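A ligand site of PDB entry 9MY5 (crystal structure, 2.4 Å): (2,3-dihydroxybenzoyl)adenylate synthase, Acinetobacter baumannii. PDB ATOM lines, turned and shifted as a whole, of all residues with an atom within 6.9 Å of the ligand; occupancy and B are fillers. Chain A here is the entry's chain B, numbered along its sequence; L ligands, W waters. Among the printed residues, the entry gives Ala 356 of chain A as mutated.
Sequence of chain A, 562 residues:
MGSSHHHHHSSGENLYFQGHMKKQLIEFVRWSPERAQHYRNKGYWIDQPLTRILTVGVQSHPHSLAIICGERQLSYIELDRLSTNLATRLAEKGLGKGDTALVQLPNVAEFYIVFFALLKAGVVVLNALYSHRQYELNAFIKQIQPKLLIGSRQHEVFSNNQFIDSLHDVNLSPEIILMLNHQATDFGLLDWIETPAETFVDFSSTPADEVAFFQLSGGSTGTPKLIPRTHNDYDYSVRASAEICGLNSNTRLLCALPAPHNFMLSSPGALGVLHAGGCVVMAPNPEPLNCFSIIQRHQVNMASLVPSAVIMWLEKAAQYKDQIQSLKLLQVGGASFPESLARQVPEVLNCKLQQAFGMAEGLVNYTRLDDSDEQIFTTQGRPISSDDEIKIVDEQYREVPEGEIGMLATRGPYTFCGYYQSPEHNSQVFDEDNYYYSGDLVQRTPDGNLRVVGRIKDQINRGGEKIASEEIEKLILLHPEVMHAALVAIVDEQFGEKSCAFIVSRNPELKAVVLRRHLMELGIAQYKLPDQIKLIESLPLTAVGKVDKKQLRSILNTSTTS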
ATOM      1  N   LEU A 216     -30.770  28.634  17.584  1.00  0.00           N
ATOM      2  CA  LEU A 216     -29.795  29.444  16.847  1.00  0.00           C
ATOM      3  C   LEU A 216     -28.414  28.858  17.039  1.00  0.00           C
ATOM      4  O   LEU A 216     -28.042  28.482  18.156  1.00  0.00           O
ATOM      5  CB  LEU A 216     -29.801  30.910  17.303  1.00  0.00           C
ATOM      6  CG  LEU A 216     -31.098  31.706  17.066  1.00  0.00           C
ATOM      7  CD1 LEU A 216     -30.972  33.135  17.544  1.00  0.00           C
ATOM      8  CD2 LEU A 216     -31.457  31.644  15.595  1.00  0.00           C
ATOM      9  N   GLY A 218     -24.420  28.580  17.581  1.00  0.00           N
ATOM     10  CA  GLY A 218     -23.362  29.314  18.262  1.00  0.00           C
ATOM     11  C   GLY A 218     -22.045  29.145  17.509  1.00  0.00           C
ATOM     12  O   GLY A 218     -21.718  28.055  17.031  1.00  0.00           O
ATOM     13  N   HIS A 261     -31.224  30.908  25.297  1.00  0.00           N
ATOM     14  CA  HIS A 261     -30.088  30.067  24.924  1.00  0.00           C
ATOM     15  C   HIS A 261     -30.334  28.595  25.254  1.00  0.00           C
ATOM     16  O   HIS A 261     -30.874  28.261  26.315  1.00  0.00           O
ATOM     17  CB  HIS A 261     -28.815  30.535  25.635  1.00  0.00           C
ATOM     18  CG  HIS A 261     -27.577  29.930  25.072  1.00  0.00           C
ATOM     19  ND1 HIS A 261     -27.171  28.650  25.371  1.00  0.00           N
ATOM     20  CD2 HIS A 261     -26.659  30.428  24.203  1.00  0.00           C
ATOM     21  CE1 HIS A 261     -26.048  28.387  24.725  1.00  0.00           C
ATOM     22  NE2 HIS A 261     -25.731  29.441  23.986  1.00  0.00           N
ATOM     23  N   ASN A 262     -29.934  27.699  24.347  1.00  0.00           N
ATOM     24  CA  ASN A 262     -30.170  26.280  24.546  1.00  0.00           C
ATOM     25  C   ASN A 262     -29.751  25.839  25.943  1.00  0.00           C
ATOM     26  O   ASN A 262     -30.452  25.051  26.593  1.00  0.00           O
ATOM     27  CB  ASN A 262     -29.425  25.452  23.491  1.00  0.00           C
ATOM     28  CG  ASN A 262     -29.976  24.039  23.347  1.00  0.00           C
ATOM     29  OD1 ASN A 262     -31.181  23.848  23.192  1.00  0.00           O
ATOM     30  ND2 ASN A 262     -29.095  23.037  23.364  1.00  0.00           N
ATOM     31  N   PHE A 263     -28.613  26.352  26.414  1.00  0.00           N
ATOM     32  CA  PHE A 263     -28.100  25.974  27.726  1.00  0.00           C
ATOM     33  C   PHE A 263     -29.086  26.352  28.823  1.00  0.00           C
ATOM     34  O   PHE A 263     -29.411  25.535  29.690  1.00  0.00           O
ATOM     35  CB  PHE A 263     -26.739  26.663  27.932  1.00  0.00           C
ATOM     36  CG  PHE A 263     -25.991  26.246  29.189  1.00  0.00           C
ATOM     37  CD1 PHE A 263     -26.407  25.161  29.949  1.00  0.00           C
ATOM     38  CD2 PHE A 263     -24.869  26.951  29.588  1.00  0.00           C
ATOM     39  CE1 PHE A 263     -25.715  24.783  31.109  1.00  0.00           C
ATOM     40  CE2 PHE A 263     -24.158  26.589  30.770  1.00  0.00           C
ATOM     41  CZ  PHE A 263     -24.574  25.509  31.521  1.00  0.00           C
ATOM     42  N   MET A 264     -29.591  27.571  28.773  1.00  0.00           N
ATOM     43  CA  MET A 264     -30.460  28.071  29.833  1.00  0.00           C
ATOM     44  C   MET A 264     -31.909  27.640  29.682  1.00  0.00           C
ATOM     45  O   MET A 264     -32.651  27.683  30.676  1.00  0.00           O
ATOM     46  CB  MET A 264     -30.349  29.588  29.883  1.00  0.00           C
ATOM     47  CG  MET A 264     -31.023  30.194  31.066  1.00  0.00           C
ATOM     48  SD  MET A 264     -29.920  30.041  32.526  1.00  0.00           S
ATOM     49  CE  MET A 264     -30.540  28.502  33.236  1.00  0.00           C
ATOM     50  N   SER A 266     -32.977  24.476  28.190  1.00  0.00           N
ATOM     51  CA  SER A 266     -33.232  23.048  28.079  1.00  0.00           C
ATOM     52  C   SER A 266     -32.171  22.101  28.642  1.00  0.00           C
ATOM     53  O   SER A 266     -32.400  20.891  28.592  1.00  0.00           O
ATOM     54  CB  SER A 266     -33.460  22.677  26.606  1.00  0.00           C
ATOM     55  OG  SER A 266     -32.226  22.654  25.924  1.00  0.00           O
ATOM     56  N   SER A 267     -31.032  22.575  29.161  1.00  0.00           N
ATOM     57  CA  SER A 267     -29.936  21.671  29.542  1.00  0.00           C
ATOM     58  C   SER A 267     -29.407  21.983  30.940  1.00  0.00           C
ATOM     59  O   SER A 267     -28.247  22.407  31.104  1.00  0.00           O
ATOM     60  CB  SER A 267     -28.785  21.722  28.537  1.00  0.00           C
ATOM     61  OG  SER A 267     -29.185  22.278  27.304  1.00  0.00           O
ATOM     62  N   PRO A 268     -30.215  21.765  31.972  1.00  0.00           N
ATOM     63  CA  PRO A 268     -31.615  21.337  31.907  1.00  0.00           C
ATOM     64  C   PRO A 268     -32.518  22.550  31.747  1.00  0.00           C
ATOM     65  O   PRO A 268     -33.604  22.462  31.170  1.00  0.00           O
ATOM     66  CB  PRO A 268     -31.814  20.583  33.229  1.00  0.00           C
ATOM     67  CG  PRO A 268     -30.912  21.322  34.183  1.00  0.00           C
ATOM     68  CD  PRO A 268     -29.707  21.725  33.357  1.00  0.00           C
ATOM     69  N   VAL A 306     -21.674  30.141  32.245  1.00  0.00           N
ATOM     70  CA  VAL A 306     -20.542  29.997  31.344  1.00  0.00           C
ATOM     71  C   VAL A 306     -19.272  30.365  32.111  1.00  0.00           C
ATOM     72  O   VAL A 306     -19.352  31.107  33.086  1.00  0.00           O
ATOM     73  CB  VAL A 306     -20.701  30.888  30.105  1.00  0.00           C
ATOM     74  CG1 VAL A 306     -21.911  30.435  29.303  1.00  0.00           C
ATOM     75  CG2 VAL A 306     -20.803  32.343  30.548  1.00  0.00           C
ATOM     76  N   GLN A 331     -24.120  24.032  37.108  1.00  0.00           N
ATOM     77  CA  GLN A 331     -23.672  23.638  35.781  1.00  0.00           C
ATOM     78  C   GLN A 331     -22.716  24.685  35.230  1.00  0.00           C
ATOM     79  O   GLN A 331     -22.968  25.895  35.343  1.00  0.00           O
ATOM     80  CB  GLN A 331     -24.854  23.473  34.814  1.00  0.00           C
ATOM     81  CG  GLN A 331     -25.774  22.257  34.950  1.00  0.00           C
ATOM     82  CD  GLN A 331     -26.928  22.536  35.873  1.00  0.00           C
ATOM     83  OE1 GLN A 331     -27.227  21.734  36.774  1.00  0.00           O
ATOM     84  NE2 GLN A 331     -27.568  23.701  35.688  1.00  0.00           N
ATOM     85  N   VAL A 332     -21.620  24.246  34.617  1.00  0.00           N
ATOM     86  CA  VAL A 332     -20.708  25.130  33.908  1.00  0.00           C
ATOM     87  C   VAL A 332     -20.429  24.558  32.522  1.00  0.00           C
ATOM     88  O   VAL A 332     -20.048  23.385  32.394  1.00  0.00           O
ATOM     89  CB  VAL A 332     -19.375  25.348  34.660  1.00  0.00           C
ATOM     90  CG1 VAL A 332     -18.464  26.223  33.840  1.00  0.00           C
ATOM     91  CG2 VAL A 332     -19.604  25.947  36.065  1.00  0.00           C
ATOM     92  N   GLY A 333     -20.602  25.386  31.501  1.00  0.00           N
ATOM     93  CA  GLY A 333     -20.215  24.979  30.162  1.00  0.00           C
ATOM     94  C   GLY A 333     -20.293  26.173  29.226  1.00  0.00           C
ATOM     95  O   GLY A 333     -20.727  27.264  29.606  1.00  0.00           O
ATOM     96  N   GLY A 334     -19.871  25.938  27.993  1.00  0.00           N
ATOM     97  CA  GLY A 334     -19.974  26.940  26.951  1.00  0.00           C
ATOM     98  C   GLY A 334     -18.636  27.462  26.485  1.00  0.00           C
ATOM     99  O   GLY A 334     -18.599  28.184  25.472  1.00  0.00           O
ATOM    100  N   ALA A 335     -17.555  27.110  27.160  1.00  0.00           N
ATOM    101  CA  ALA A 335     -16.227  27.647  26.853  1.00  0.00           C
ATOM    102  C   ALA A 335     -15.237  26.872  27.701  1.00  0.00           C
ATOM    103  O   ALA A 335     -15.604  26.182  28.654  1.00  0.00           O
ATOM    104  CB  ALA A 335     -16.126  29.155  27.130  1.00  0.00           C
ATOM    105  N   ALA A 356     -20.681  20.652  31.631  1.00  0.00           N
ATOM    106  CA  ALA A 356     -21.511  20.315  30.490  1.00  0.00           C
ATOM    107  C   ALA A 356     -20.858  20.866  29.239  1.00  0.00           C
ATOM    108  O   ALA A 356     -20.135  21.876  29.281  1.00  0.00           O
ATOM    109  CB  ALA A 356     -22.939  20.855  30.640  1.00  0.00           C
ATOM    110  N   PHE A 357     -21.093  20.171  28.144  1.00  0.00           N
ATOM    111  CA  PHE A 357     -20.672  20.597  26.827  1.00  0.00           C
ATOM    112  C   PHE A 357     -21.795  20.217  25.886  1.00  0.00           C
ATOM    113  O   PHE A 357     -22.079  19.025  25.704  1.00  0.00           O
ATOM    114  CB  PHE A 357     -19.351  19.924  26.426  1.00  0.00           C
ATOM    115  CG  PHE A 357     -19.163  19.853  24.949  1.00  0.00           C
ATOM    116  CD1 PHE A 357     -19.226  21.004  24.186  1.00  0.00           C
ATOM    117  CD2 PHE A 357     -18.942  18.638  24.330  1.00  0.00           C
ATOM    118  CE1 PHE A 357     -19.056  20.957  22.815  1.00  0.00           C
ATOM    119  CE2 PHE A 357     -18.778  18.567  22.945  1.00  0.00           C
ATOM    120  CZ  PHE A 357     -18.838  19.730  22.189  1.00  0.00           C
ATOM    121  N   GLY A 358     -22.475  21.219  25.346  1.00  0.00           N
ATOM    122  CA  GLY A 358     -23.612  20.996  24.499  1.00  0.00           C
ATOM    123  C   GLY A 358     -23.576  21.935  23.312  1.00  0.00           C
ATOM    124  O   GLY A 358     -22.643  22.727  23.145  1.00  0.00           O
ATOM    125  N   MET A 359     -24.613  21.836  22.499  1.00  0.00           N
ATOM    126  CA  MET A 359     -24.726  22.651  21.310  1.00  0.00           C
ATOM    127  C   MET A 359     -26.208  22.776  20.999  1.00  0.00           C
ATOM    128  O   MET A 359     -26.979  21.838  21.230  1.00  0.00           O
ATOM    129  CB  MET A 359     -23.945  22.037  20.141  1.00  0.00           C
ATOM    130  CG  MET A 359     -24.429  20.633  19.749  1.00  0.00           C
ATOM    131  SD  MET A 359     -23.318  19.792  18.571  1.00  0.00           S
ATOM    132  CE  MET A 359     -21.900  19.461  19.618  1.00  0.00           C
ATOM    133  N   ALA A 360     -26.604  23.950  20.509  1.00  0.00           N
ATOM    134  CA  ALA A 360     -28.002  24.148  20.154  1.00  0.00           C
ATOM    135  C   ALA A 360     -28.450  23.239  19.011  1.00  0.00           C
ATOM    136  O   ALA A 360     -29.651  23.089  18.787  1.00  0.00           O
ATOM    137  CB  ALA A 360     -28.221  25.622  19.784  1.00  0.00           C
ATOM    138  N   GLU A 361     -27.517  22.645  18.260  1.00  0.00           N
ATOM    139  CA  GLU A 361     -27.864  21.715  17.192  1.00  0.00           C
ATOM    140  C   GLU A 361     -28.357  20.381  17.752  1.00  0.00           C
ATOM    141  O   GLU A 361     -29.031  19.627  17.037  1.00  0.00           O
ATOM    142  CB  GLU A 361     -26.654  21.491  16.295  1.00  0.00           C
ATOM    143  CG  GLU A 361     -26.363  22.631  15.314  1.00  0.00           C
ATOM    144  CD  GLU A 361     -25.542  23.785  15.928  1.00  0.00           C
ATOM    145  OE1 GLU A 361     -25.244  23.757  17.155  1.00  0.00           O
ATOM    146  OE2 GLU A 361     -25.167  24.701  15.169  1.00  0.00           O
ATOM    147  N   GLY A 362     -28.039  20.087  19.019  1.00  0.00           N
ATOM    148  CA  GLY A 362     -28.497  18.843  19.612  1.00  0.00           C
ATOM    149  C   GLY A 362     -27.674  18.327  20.779  1.00  0.00           C
ATOM    150  O   GLY A 362     -27.886  18.726  21.926  1.00  0.00           O
ATOM    151  N   LEU A 363     -26.735  17.419  20.483  1.00  0.00           N
ATOM    152  CA  LEU A 363     -25.911  16.742  21.472  1.00  0.00           C
ATOM    153  C   LEU A 363     -25.593  17.595  22.690  1.00  0.00           C
ATOM    154  O   LEU A 363     -25.078  18.729  22.572  1.00  0.00           O
ATOM    155  CB  LEU A 363     -24.597  16.286  20.816  1.00  0.00           C
ATOM    156  CG  LEU A 363     -23.542  15.607  21.702  1.00  0.00           C
ATOM    157  CD1 LEU A 363     -24.160  14.376  22.351  1.00  0.00           C
ATOM    158  CD2 LEU A 363     -22.318  15.215  20.880  1.00  0.00           C
ATOM    159  N   VAL A 364     -25.860  17.044  23.873  1.00  0.00           N
ATOM    160  CA  VAL A 364     -25.506  17.664  25.141  1.00  0.00           C
ATOM    161  C   VAL A 364     -24.811  16.612  25.991  1.00  0.00           C
ATOM    162  O   VAL A 364     -25.306  15.473  26.095  1.00  0.00           O
ATOM    163  CB  VAL A 364     -26.745  18.222  25.862  1.00  0.00           C
ATOM    164  CG1 VAL A 364     -26.346  18.713  27.254  1.00  0.00           C
ATOM    165  CG2 VAL A 364     -27.383  19.336  25.029  1.00  0.00           C
ATOM    166  N   ASN A 365     -23.676  16.974  26.583  1.00  0.00           N
ATOM    167  CA  ASN A 365     -22.921  16.122  27.498  1.00  0.00           C
ATOM    168  C   ASN A 365     -22.919  16.716  28.903  1.00  0.00           C
ATOM    169  O   ASN A 365     -22.748  17.929  29.067  1.00  0.00           O
ATOM    170  CB  ASN A 365     -21.469  15.962  27.063  1.00  0.00           C
ATOM    171  CG  ASN A 365     -21.329  15.463  25.653  1.00  0.00           C
ATOM    172  OD1 ASN A 365     -21.254  14.267  25.421  1.00  0.00           O
ATOM    173  ND2 ASN A 365     -21.267  16.391  24.695  1.00  0.00           N
ATOM    174  N   TYR A 366     -23.086  15.860  29.909  1.00  0.00           N
ATOM    175  CA  TYR A 366     -22.943  16.261  31.313  1.00  0.00           C
ATOM    176  C   TYR A 366     -22.021  15.290  32.051  1.00  0.00           C
ATOM    177  O   TYR A 366     -22.060  14.079  31.791  1.00  0.00           O
ATOM    178  CB  TYR A 366     -24.283  16.280  32.056  1.00  0.00           C
ATOM    179  CG  TYR A 366     -25.405  17.083  31.450  1.00  0.00           C
ATOM    180  CD1 TYR A 366     -25.547  18.436  31.701  1.00  0.00           C
ATOM    181  CD2 TYR A 366     -26.383  16.450  30.671  1.00  0.00           C
ATOM    182  CE1 TYR A 366     -26.609  19.162  31.169  1.00  0.00           C
ATOM    183  CE2 TYR A 366     -27.448  17.158  30.140  1.00  0.00           C
ATOM    184  CZ  TYR A 366     -27.567  18.518  30.386  1.00  0.00           C
ATOM    185  OH  TYR A 366     -28.649  19.187  29.830  1.00  0.00           O
HETATM  186  C1  LIG L   1     -25.540  22.100  28.303  1.00  0.00           C
HETATM  187  C2  LIG L   1     -25.042  23.074  27.237  1.00  0.00           C
HETATM  188  C3  LIG L   1     -25.795  23.228  26.079  1.00  0.00           C
HETATM  189  C4  LIG L   1     -25.360  24.111  25.118  1.00  0.00           C
HETATM  190  C5  LIG L   1     -24.189  24.831  25.307  1.00  0.00           C
HETATM  191  C6  LIG L   1     -23.446  24.667  26.470  1.00  0.00           C
HETATM  192  C7  LIG L   1     -23.872  23.789  27.435  1.00  0.00           C
HETATM  193  C8  LIG L   1     -23.715  25.801  24.214  1.00  0.00           C
HETATM  194  O1  LIG L   1     -22.715  26.547  24.373  1.00  0.00           O
HETATM  195  O2  LIG L   1     -24.349  25.848  23.116  1.00  0.00           O
HETATM  196  O3  LIG L   1     -26.126  24.273  23.953  1.00  0.00           O
HETATM  197  O   HOH W   1     -20.921  24.143  25.255  1.00  0.00           O
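The backbone NH (N) of Met 359 lies within hydrogen-bond range of an oxygen (O3) of the ligand, at 3.2 Å. O3 of the ligand lies within hydrogen-bond range of ND2 of Asn 262 (3.3 Å). O3 of the ligand sits at hydrogen-bond distance from N of Ala 360 (3.5 Å).
The side-chain amide nitrogen (ND2) of Asn 262 lies within hydrogen-bond range of the backbone carbonyl oxygen (O) of Met 359. The backbone carbonyl oxygen (O) of Asn 262 lies within hydrogen-bond range of the side-chain hydroxyl (OG) of Ser 267. O of Asn 262 is in hydrogen-bond range of OG of Ser 266. OH of Tyr 366 lies close to O of Ser 267 (3.5 Å). OG of Ser 266 lies close to OG of Ser 267, at 3.4 Å. The backbone NH (N) of Phe 263 lies within hydrogen-bond range of a ring nitrogen (ND1) of His 261 (2.9 Å). The backbone NH of Ala 356 lies within hydrogen-bond range of the backbone carbonyl oxygen of Val 332, 2.9 Å away.
Merely in contact with the ligand: His 261 (3.5 Å), Phe 263 (3.6 Å), Ser 267 (3.3 Å), Gly 334 (3.8 Å), Ala 356 (3.7 Å), Gly 358 (3.3 Å) and Val 364 (3.6 Å). Hydrophobic or aromatic side chains within 4 Å of the ligand: His 261, Phe 263, Ala 356 and Val 364. Ten residues have an atom within 4 Å of the ligand: His 261, Asn 262, Phe 263, Ser 267, Gly 334, Ala 356, Gly 358, Met 359, Ala 360 and Val 364.
Water W1 lies within hydrogen-bond range of the backbone carbonyl oxygen (O) of Gly 358 (3.1 Å), an oxygen (O1) of the ligand (3.1 Å) and the backbone NH (N) of Gly 334 (3.4 Å).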
